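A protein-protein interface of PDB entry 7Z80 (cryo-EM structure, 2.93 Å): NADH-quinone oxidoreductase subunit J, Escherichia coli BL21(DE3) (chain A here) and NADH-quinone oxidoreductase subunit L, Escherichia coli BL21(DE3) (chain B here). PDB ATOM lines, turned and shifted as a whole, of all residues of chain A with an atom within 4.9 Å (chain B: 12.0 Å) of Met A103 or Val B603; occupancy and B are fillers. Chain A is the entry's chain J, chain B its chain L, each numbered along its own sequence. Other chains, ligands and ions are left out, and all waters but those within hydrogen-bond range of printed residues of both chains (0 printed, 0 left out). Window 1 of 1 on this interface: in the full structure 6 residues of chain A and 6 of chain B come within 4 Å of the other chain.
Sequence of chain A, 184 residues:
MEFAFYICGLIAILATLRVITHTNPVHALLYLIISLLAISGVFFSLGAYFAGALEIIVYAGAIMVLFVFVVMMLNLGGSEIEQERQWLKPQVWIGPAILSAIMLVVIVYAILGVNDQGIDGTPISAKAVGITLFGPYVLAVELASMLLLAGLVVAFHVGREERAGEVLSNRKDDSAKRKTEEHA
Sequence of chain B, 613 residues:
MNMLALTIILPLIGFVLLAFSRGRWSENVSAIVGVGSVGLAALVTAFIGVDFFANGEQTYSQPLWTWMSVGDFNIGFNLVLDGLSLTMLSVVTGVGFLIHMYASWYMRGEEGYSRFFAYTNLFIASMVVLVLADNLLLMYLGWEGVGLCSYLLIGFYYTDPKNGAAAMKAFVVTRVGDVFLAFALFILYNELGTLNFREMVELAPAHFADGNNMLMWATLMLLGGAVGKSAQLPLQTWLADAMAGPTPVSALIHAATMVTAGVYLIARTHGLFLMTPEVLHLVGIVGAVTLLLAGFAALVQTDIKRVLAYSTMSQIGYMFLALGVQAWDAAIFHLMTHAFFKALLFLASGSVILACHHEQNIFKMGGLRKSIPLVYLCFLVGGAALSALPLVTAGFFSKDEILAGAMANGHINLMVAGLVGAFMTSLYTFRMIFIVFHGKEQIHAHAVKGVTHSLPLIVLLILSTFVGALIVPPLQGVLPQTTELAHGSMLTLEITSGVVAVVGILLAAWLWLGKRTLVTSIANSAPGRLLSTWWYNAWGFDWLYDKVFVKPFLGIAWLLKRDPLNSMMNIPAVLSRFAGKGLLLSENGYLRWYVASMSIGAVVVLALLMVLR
The backbone carbonyl oxygen (O) of Val B595 lies within hydrogen-bond range of the side-chain hydroxyl (OG) of Ser B599, 2.9 Å away.
Of the 20 printed residues of chain B, 5 touch a printed residue of chain A. Hydrophobic or aromatic side chains of chain B within 4 Å of the printed part of chain A: Ile B600, Val B603 and Leu B606.
No residue of chain B comes within 4 Å of Ser A100. Of chain B, only Val B603 (3.9 Å) comes within 4 Å of Ile A102. Met A103 touches just one residue of chain B: Val B603 (3.7 Å). No residue of chain B comes within 4 Å of Val A105. Val A106 touches just one residue of chain B: Leu B606 (3.7 Å). Printed residues of chain B within 4 Å of Ile A107: Leu B606 (3.9 Å). Printed residues of chain A within 4 Å of Ala B596: Leu A99 (3.8 Å). Of the printed residues of chain A, Ser B599 touches Leu A99. Of the printed residues of chain A, Ile B600 touches Leu A99 (3.7 Å).
O of Ala B596 touches CD2 of Leu A99 (3.8 Å). Leu A99 touches Ser B599. CG1 of Ile B600 touches CD2 of Leu A99, 3.7 Å away. Val B603 touches Leu A99 (CG2 to CD1, 3.9 Å). Val B603 touches Ile A102. CB of Met A103 touches CG2 of Val B603 (3.7 Å). CG1 of Val A106 touches CB of Leu B606 (3.7 Å). Ile A107 touches Leu B606.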
ATOM      1  N   ILE A  98     -19.104  18.915  23.051  1.00  0.00           N
ATOM      2  CA  ILE A  98     -17.765  19.489  23.142  1.00  0.00           C
ATOM      3  C   ILE A  98     -17.385  20.195  21.844  1.00  0.00           C
ATOM      4  O   ILE A  98     -16.656  21.195  21.868  1.00  0.00           O
ATOM      5  CB  ILE A  98     -16.741  18.407  23.546  1.00  0.00           C
ATOM      6  CG1 ILE A  98     -16.635  17.308  22.478  1.00  0.00           C
ATOM      7  CG2 ILE A  98     -17.098  17.833  24.915  1.00  0.00           C
ATOM      8  CD1 ILE A  98     -16.006  16.010  22.958  1.00  0.00           C
ATOM      9  N   LEU A  99     -17.892  19.717  20.704  1.00  0.00           N
ATOM     10  CA  LEU A  99     -17.656  20.392  19.431  1.00  0.00           C
ATOM     11  C   LEU A  99     -18.337  21.754  19.394  1.00  0.00           C
ATOM     12  O   LEU A  99     -17.732  22.751  18.975  1.00  0.00           O
ATOM     13  CB  LEU A  99     -18.153  19.512  18.287  1.00  0.00           C
ATOM     14  CG  LEU A  99     -17.840  19.937  16.856  1.00  0.00           C
ATOM     15  CD1 LEU A  99     -16.346  19.890  16.593  1.00  0.00           C
ATOM     16  CD2 LEU A  99     -18.589  19.037  15.894  1.00  0.00           C
ATOM     17  N   SER A 100     -19.591  21.816  19.850  1.00  0.00           N
ATOM     18  CA  SER A 100     -20.291  23.093  19.929  1.00  0.00           C
ATOM     19  C   SER A 100     -19.620  24.027  20.928  1.00  0.00           C
ATOM     20  O   SER A 100     -19.540  25.238  20.695  1.00  0.00           O
ATOM     21  CB  SER A 100     -21.753  22.868  20.304  1.00  0.00           C
ATOM     22  OG  SER A 100     -21.861  22.122  21.503  1.00  0.00           O
ATOM     23  N   ALA A 101     -19.108  23.479  22.034  1.00  0.00           N
ATOM     24  CA  ALA A 101     -18.433  24.302  23.033  1.00  0.00           C
ATOM     25  C   ALA A 101     -17.128  24.888  22.500  1.00  0.00           C
ATOM     26  O   ALA A 101     -16.843  26.073  22.720  1.00  0.00           O
ATOM     27  CB  ALA A 101     -18.174  23.483  24.297  1.00  0.00           C
ATOM     28  N   ILE A 102     -16.317  24.081  21.807  1.00  0.00           N
ATOM     29  CA  ILE A 102     -15.052  24.596  21.287  1.00  0.00           C
ATOM     30  C   ILE A 102     -15.303  25.587  20.151  1.00  0.00           C
ATOM     31  O   ILE A 102     -14.596  26.596  20.030  1.00  0.00           O
ATOM     32  CB  ILE A 102     -14.103  23.443  20.883  1.00  0.00           C
ATOM     33  CG1 ILE A 102     -12.693  23.968  20.594  1.00  0.00           C
ATOM     34  CG2 ILE A 102     -14.610  22.638  19.698  1.00  0.00           C
ATOM     35  CD1 ILE A 102     -11.989  24.537  21.804  1.00  0.00           C
ATOM     36  N   MET A 103     -16.344  25.354  19.339  1.00  0.00           N
ATOM     37  CA  MET A 103     -16.716  26.333  18.321  1.00  0.00           C
ATOM     38  C   MET A 103     -17.173  27.641  18.952  1.00  0.00           C
ATOM     39  O   MET A 103     -16.798  28.727  18.491  1.00  0.00           O
ATOM     40  CB  MET A 103     -17.815  25.767  17.431  1.00  0.00           C
ATOM     41  CG  MET A 103     -18.239  26.684  16.306  1.00  0.00           C
ATOM     42  SD  MET A 103     -18.968  25.718  14.984  1.00  0.00           S
ATOM     43  CE  MET A 103     -20.309  24.980  15.903  1.00  0.00           C
ATOM     44  N   LEU A 104     -17.976  27.554  20.017  1.00  0.00           N
ATOM     45  CA  LEU A 104     -18.462  28.747  20.695  1.00  0.00           C
ATOM     46  C   LEU A 104     -17.321  29.532  21.325  1.00  0.00           C
ATOM     47  O   LEU A 104     -17.303  30.764  21.259  1.00  0.00           O
ATOM     48  CB  LEU A 104     -19.497  28.364  21.750  1.00  0.00           C
ATOM     49  CG  LEU A 104     -20.188  29.519  22.476  1.00  0.00           C
ATOM     50  CD1 LEU A 104     -20.828  30.471  21.480  1.00  0.00           C
ATOM     51  CD2 LEU A 104     -21.220  28.989  23.455  1.00  0.00           C
ATOM     52  N   VAL A 105     -16.351  28.840  21.929  1.00  0.00           N
ATOM     53  CA  VAL A 105     -15.252  29.568  22.558  1.00  0.00           C
ATOM     54  C   VAL A 105     -14.310  30.157  21.505  1.00  0.00           C
ATOM     55  O   VAL A 105     -13.738  31.233  21.719  1.00  0.00           O
ATOM     56  CB  VAL A 105     -14.521  28.685  23.594  1.00  0.00           C
ATOM     57  CG1 VAL A 105     -13.604  27.666  22.947  1.00  0.00           C
ATOM     58  CG2 VAL A 105     -13.751  29.552  24.583  1.00  0.00           C
ATOM     59  N   VAL A 106     -14.172  29.511  20.339  1.00  0.00           N
ATOM     60  CA  VAL A 106     -13.381  30.102  19.259  1.00  0.00           C
ATOM     61  C   VAL A 106     -14.060  31.363  18.726  1.00  0.00           C
ATOM     62  O   VAL A 106     -13.409  32.396  18.510  1.00  0.00           O
ATOM     63  CB  VAL A 106     -13.134  29.062  18.148  1.00  0.00           C
ATOM     64  CG1 VAL A 106     -12.697  29.732  16.859  1.00  0.00           C
ATOM     65  CG2 VAL A 106     -12.076  28.066  18.588  1.00  0.00           C
ATOM     66  N   ILE A 107     -15.382  31.309  18.539  1.00  0.00           N
ATOM     67  CA  ILE A 107     -16.113  32.479  18.060  1.00  0.00           C
ATOM     68  C   ILE A 107     -16.101  33.592  19.110  1.00  0.00           C
ATOM     69  O   ILE A 107     -16.029  34.778  18.771  1.00  0.00           O
ATOM     70  CB  ILE A 107     -17.542  32.077  17.642  1.00  0.00           C
ATOM     71  CG1 ILE A 107     -17.491  31.123  16.449  1.00  0.00           C
ATOM     72  CG2 ILE A 107     -18.361  33.284  17.231  1.00  0.00           C
ATOM     73  CD1 ILE A 107     -18.847  30.618  16.007  1.00  0.00           C
ATOM     74  N   ARG B 592     -26.815  13.331   9.789  1.00  0.00           N
ATOM     75  CA  ARG B 592     -26.316  13.928  11.024  1.00  0.00           C
ATOM     76  C   ARG B 592     -24.796  13.870  11.084  1.00  0.00           C
ATOM     77  O   ARG B 592     -24.152  14.799  11.588  1.00  0.00           O
ATOM     78  CB  ARG B 592     -26.933  13.226  12.231  1.00  0.00           C
ATOM     79  CG  ARG B 592     -28.452  13.212  12.220  1.00  0.00           C
ATOM     80  CD  ARG B 592     -29.022  12.888  13.590  1.00  0.00           C
ATOM     81  NE  ARG B 592     -28.663  11.548  14.036  1.00  0.00           N
ATOM     82  CZ  ARG B 592     -27.841  11.289  15.044  1.00  0.00           C
ATOM     83  NH1 ARG B 592     -27.266  12.261  15.733  1.00  0.00           N
ATOM     84  NH2 ARG B 592     -27.591  10.025  15.370  1.00  0.00           N
ATOM     85  N   TYR B 594     -22.975  14.075   8.396  1.00  0.00           N
ATOM     86  CA  TYR B 594     -22.556  15.112   7.454  1.00  0.00           C
ATOM     87  C   TYR B 594     -22.573  16.492   8.102  1.00  0.00           C
ATOM     88  O   TYR B 594     -21.645  17.289   7.907  1.00  0.00           O
ATOM     89  CB  TYR B 594     -23.448  15.093   6.212  1.00  0.00           C
ATOM     90  CG  TYR B 594     -23.285  13.875   5.323  1.00  0.00           C
ATOM     91  CD1 TYR B 594     -22.222  12.996   5.492  1.00  0.00           C
ATOM     92  CD2 TYR B 594     -24.191  13.617   4.304  1.00  0.00           C
ATOM     93  CE1 TYR B 594     -22.074  11.888   4.680  1.00  0.00           C
ATOM     94  CE2 TYR B 594     -24.048  12.513   3.485  1.00  0.00           C
ATOM     95  CZ  TYR B 594     -22.989  11.655   3.677  1.00  0.00           C
ATOM     96  OH  TYR B 594     -22.842  10.555   2.864  1.00  0.00           O
ATOM     97  N   VAL B 595     -23.608  16.782   8.895  1.00  0.00           N
ATOM     98  CA  VAL B 595     -23.668  18.064   9.596  1.00  0.00           C
ATOM     99  C   VAL B 595     -22.574  18.152  10.657  1.00  0.00           C
ATOM    100  O   VAL B 595     -21.951  19.208  10.843  1.00  0.00           O
ATOM    101  CB  VAL B 595     -25.068  18.277  10.197  1.00  0.00           C
ATOM    102  CG1 VAL B 595     -25.173  19.654  10.799  1.00  0.00           C
ATOM    103  CG2 VAL B 595     -26.131  18.105   9.131  1.00  0.00           C
ATOM    104  N   ALA B 596     -22.308  17.043  11.355  1.00  0.00           N
ATOM    105  CA  ALA B 596     -21.233  17.022  12.343  1.00  0.00           C
ATOM    106  C   ALA B 596     -19.870  17.216  11.687  1.00  0.00           C
ATOM    107  O   ALA B 596     -18.996  17.883  12.248  1.00  0.00           O
ATOM    108  CB  ALA B 596     -21.269  15.713  13.129  1.00  0.00           C
ATOM    109  N   SER B 597     -19.674  16.646  10.496  1.00  0.00           N
ATOM    110  CA  SER B 597     -18.416  16.823   9.779  1.00  0.00           C
ATOM    111  C   SER B 597     -18.262  18.252   9.277  1.00  0.00           C
ATOM    112  O   SER B 597     -17.148  18.788   9.253  1.00  0.00           O
ATOM    113  CB  SER B 597     -18.333  15.835   8.616  1.00  0.00           C
ATOM    114  OG  SER B 597     -19.269  16.167   7.606  1.00  0.00           O
ATOM    115  N   MET B 598     -19.368  18.882   8.867  1.00  0.00           N
ATOM    116  CA  MET B 598     -19.321  20.297   8.507  1.00  0.00           C
ATOM    117  C   MET B 598     -18.940  21.159   9.705  1.00  0.00           C
ATOM    118  O   MET B 598     -18.135  22.092   9.579  1.00  0.00           O
ATOM    119  CB  MET B 598     -20.670  20.739   7.941  1.00  0.00           C
ATOM    120  CG  MET B 598     -20.831  20.498   6.449  1.00  0.00           C
ATOM    121  SD  MET B 598     -22.102  21.514   5.662  1.00  0.00           S
ATOM    122  CE  MET B 598     -22.450  22.738   6.923  1.00  0.00           C
ATOM    123  N   SER B 599     -19.496  20.847  10.880  1.00  0.00           N
ATOM    124  CA  SER B 599     -19.129  21.573  12.095  1.00  0.00           C
ATOM    125  C   SER B 599     -17.667  21.337  12.464  1.00  0.00           C
ATOM    126  O   SER B 599     -16.972  22.265  12.900  1.00  0.00           O
ATOM    127  CB  SER B 599     -20.043  21.157  13.244  1.00  0.00           C
ATOM    128  OG  SER B 599     -21.403  21.200  12.853  1.00  0.00           O
ATOM    129  N   ILE B 600     -17.188  20.101  12.293  1.00  0.00           N
ATOM    130  CA  ILE B 600     -15.792  19.769  12.575  1.00  0.00           C
ATOM    131  C   ILE B 600     -14.866  20.558  11.658  1.00  0.00           C
ATOM    132  O   ILE B 600     -13.861  21.128  12.101  1.00  0.00           O
ATOM    133  CB  ILE B 600     -15.569  18.249  12.437  1.00  0.00           C
ATOM    134  CG1 ILE B 600     -16.072  17.512  13.677  1.00  0.00           C
ATOM    135  CG2 ILE B 600     -14.100  17.917  12.198  1.00  0.00           C
ATOM    136  CD1 ILE B 600     -16.047  16.006  13.540  1.00  0.00           C
ATOM    137  N   GLY B 601     -15.206  20.618  10.370  1.00  0.00           N
ATOM    138  CA  GLY B 601     -14.406  21.387   9.432  1.00  0.00           C
ATOM    139  C   GLY B 601     -14.422  22.875   9.722  1.00  0.00           C
ATOM    140  O   GLY B 601     -13.406  23.555   9.555  1.00  0.00           O
ATOM    141  N   ALA B 602     -15.573  23.399  10.160  1.00  0.00           N
ATOM    142  CA  ALA B 602     -15.650  24.804  10.554  1.00  0.00           C
ATOM    143  C   ALA B 602     -14.755  25.094  11.753  1.00  0.00           C
ATOM    144  O   ALA B 602     -14.038  26.105  11.772  1.00  0.00           O
ATOM    145  CB  ALA B 602     -17.097  25.184  10.859  1.00  0.00           C
ATOM    146  N   VAL B 603     -14.770  24.206  12.753  1.00  0.00           N
ATOM    147  CA  VAL B 603     -13.896  24.358  13.915  1.00  0.00           C
ATOM    148  C   VAL B 603     -12.432  24.296  13.493  1.00  0.00           C
ATOM    149  O   VAL B 603     -11.601  25.081  13.965  1.00  0.00           O
ATOM    150  CB  VAL B 603     -14.229  23.289  14.975  1.00  0.00           C
ATOM    151  CG1 VAL B 603     -13.184  23.268  16.083  1.00  0.00           C
ATOM    152  CG2 VAL B 603     -15.599  23.540  15.564  1.00  0.00           C
ATOM    153  N   VAL B 604     -12.106  23.386  12.572  1.00  0.00           N
ATOM    154  CA  VAL B 604     -10.724  23.205  12.133  1.00  0.00           C
ATOM    155  C   VAL B 604     -10.220  24.442  11.392  1.00  0.00           C
ATOM    156  O   VAL B 604      -9.118  24.937  11.666  1.00  0.00           O
ATOM    157  CB  VAL B 604     -10.607  21.930  11.276  1.00  0.00           C
ATOM    158  CG1 VAL B 604      -9.344  21.943  10.438  1.00  0.00           C
ATOM    159  CG2 VAL B 604     -10.620  20.699  12.167  1.00  0.00           C
ATOM    160  N   VAL B 605     -11.022  24.975  10.462  1.00  0.00           N
ATOM    161  CA  VAL B 605     -10.568  26.137   9.697  1.00  0.00           C
ATOM    162  C   VAL B 605     -10.514  27.379  10.586  1.00  0.00           C
ATOM    163  O   VAL B 605      -9.612  28.215  10.444  1.00  0.00           O
ATOM    164  CB  VAL B 605     -11.434  26.351   8.434  1.00  0.00           C
ATOM    165  CG1 VAL B 605     -12.886  26.629   8.765  1.00  0.00           C
ATOM    166  CG2 VAL B 605     -10.858  27.458   7.554  1.00  0.00           C
ATOM    167  N   LEU B 606     -11.441  27.501  11.545  1.00  0.00           N
ATOM    168  CA  LEU B 606     -11.397  28.636  12.463  1.00  0.00           C
ATOM    169  C   LEU B 606     -10.178  28.565  13.375  1.00  0.00           C
ATOM    170  O   LEU B 606      -9.525  29.585  13.629  1.00  0.00           O
ATOM    171  CB  LEU B 606     -12.687  28.697  13.279  1.00  0.00           C
ATOM    172  CG  LEU B 606     -13.680  29.787  12.863  1.00  0.00           C
ATOM    173  CD1 LEU B 606     -14.151  29.572  11.437  1.00  0.00           C
ATOM    174  CD2 LEU B 606     -14.865  29.821  13.813  1.00  0.00           C
ATOM    175  N   ALA B 607      -9.837  27.366  13.856  1.00  0.00           N
ATOM    176  CA  ALA B 607      -8.642  27.203  14.679  1.00  0.00           C
ATOM    177  C   ALA B 607      -7.373  27.489  13.886  1.00  0.00           C
ATOM    178  O   ALA B 607      -6.442  28.122  14.403  1.00  0.00           O
ATOM    179  CB  ALA B 607      -8.602  25.795  15.272  1.00  0.00           C
ATOM    180  N   LEU B 608      -7.315  27.036  12.627  1.00  0.00           N
ATOM    181  CA  LEU B 608      -6.152  27.330  11.796  1.00  0.00           C
ATOM    182  C   LEU B 608      -6.041  28.815  11.481  1.00  0.00           C
ATOM    183  O   LEU B 608      -4.929  29.331  11.324  1.00  0.00           O
ATOM    184  CB  LEU B 608      -6.190  26.524  10.497  1.00  0.00           C
ATOM    185  CG  LEU B 608      -5.715  25.072  10.562  1.00  0.00           C
ATOM    186  CD1 LEU B 608      -6.551  24.201   9.649  1.00  0.00           C
ATOM    187  CD2 LEU B 608      -4.243  24.975  10.197  1.00  0.00           C
ATOM    188  N   LEU B 609      -7.170  29.518  11.377  1.00  0.00           N
ATOM    189  CA  LEU B 609      -7.105  30.961  11.186  1.00  0.00           C
ATOM    190  C   LEU B 609      -6.696  31.681  12.466  1.00  0.00           C
ATOM    191  O   LEU B 609      -6.061  32.740  12.401  1.00  0.00           O
ATOM    192  CB  LEU B 609      -8.448  31.482  10.676  1.00  0.00           C
ATOM    193  CG  LEU B 609      -8.705  31.191   9.195  1.00  0.00           C
ATOM    194  CD1 LEU B 609     -10.075  31.676   8.776  1.00  0.00           C
ATOM    195  CD2 LEU B 609      -7.626  31.826   8.334  1.00  0.00           C
ATOM    196  N   MET B 610      -7.046  31.130  13.632  1.00  0.00           N
ATOM    197  CA  MET B 610      -6.665  31.773  14.888  1.00  0.00           C
ATOM    198  C   MET B 610      -5.195  31.555  15.230  1.00  0.00           C
ATOM    199  O   MET B 610      -4.557  32.448  15.799  1.00  0.00           O
ATOM    200  CB  MET B 610      -7.550  31.283  16.032  1.00  0.00           C
ATOM    201  CG  MET B 610      -8.983  31.754  15.933  1.00  0.00           C
ATOM    202  SD  MET B 610      -9.107  33.304  15.027  1.00  0.00           S
ATOM    203  CE  MET B 610     -10.878  33.469  14.914  1.00  0.00           C
ATOM    204  N   VAL B 611      -4.639  30.384  14.908  1.00  0.00           N
ATOM    205  CA  VAL B 611      -3.241  30.136  15.254  1.00  0.00           C
ATOM    206  C   VAL B 611      -2.282  30.914  14.359  1.00  0.00           C
ATOM    207  O   VAL B 611      -1.104  31.059  14.702  1.00  0.00           O
ATOM    208  CB  VAL B 611      -2.907  28.632  15.213  1.00  0.00           C
ATOM    209  CG1 VAL B 611      -3.738  27.872  16.235  1.00  0.00           C
ATOM    210  CG2 VAL B 611      -3.110  28.072  13.817  1.00  0.00           C
ATOM    211  N   LEU B 612      -2.749  31.419  13.222  1.00  0.00           N
ATOM    212  CA  LEU B 612      -1.922  32.257  12.361  1.00  0.00           C
ATOM    213  C   LEU B 612      -2.509  33.660  12.246  1.00  0.00           C
ATOM    214  O   LEU B 612      -2.333  34.336  11.234  1.00  0.00           O
ATOM    215  CB  LEU B 612      -1.775  31.632  10.972  1.00  0.00           C
ATOM    216  CG  LEU B 612      -1.738  30.104  10.905  1.00  0.00           C
ATOM    217  CD1 LEU B 612      -2.057  29.621   9.499  1.00  0.00           C
ATOM    218  CD2 LEU B 612      -0.387  29.581  11.361  1.00  0.00           C
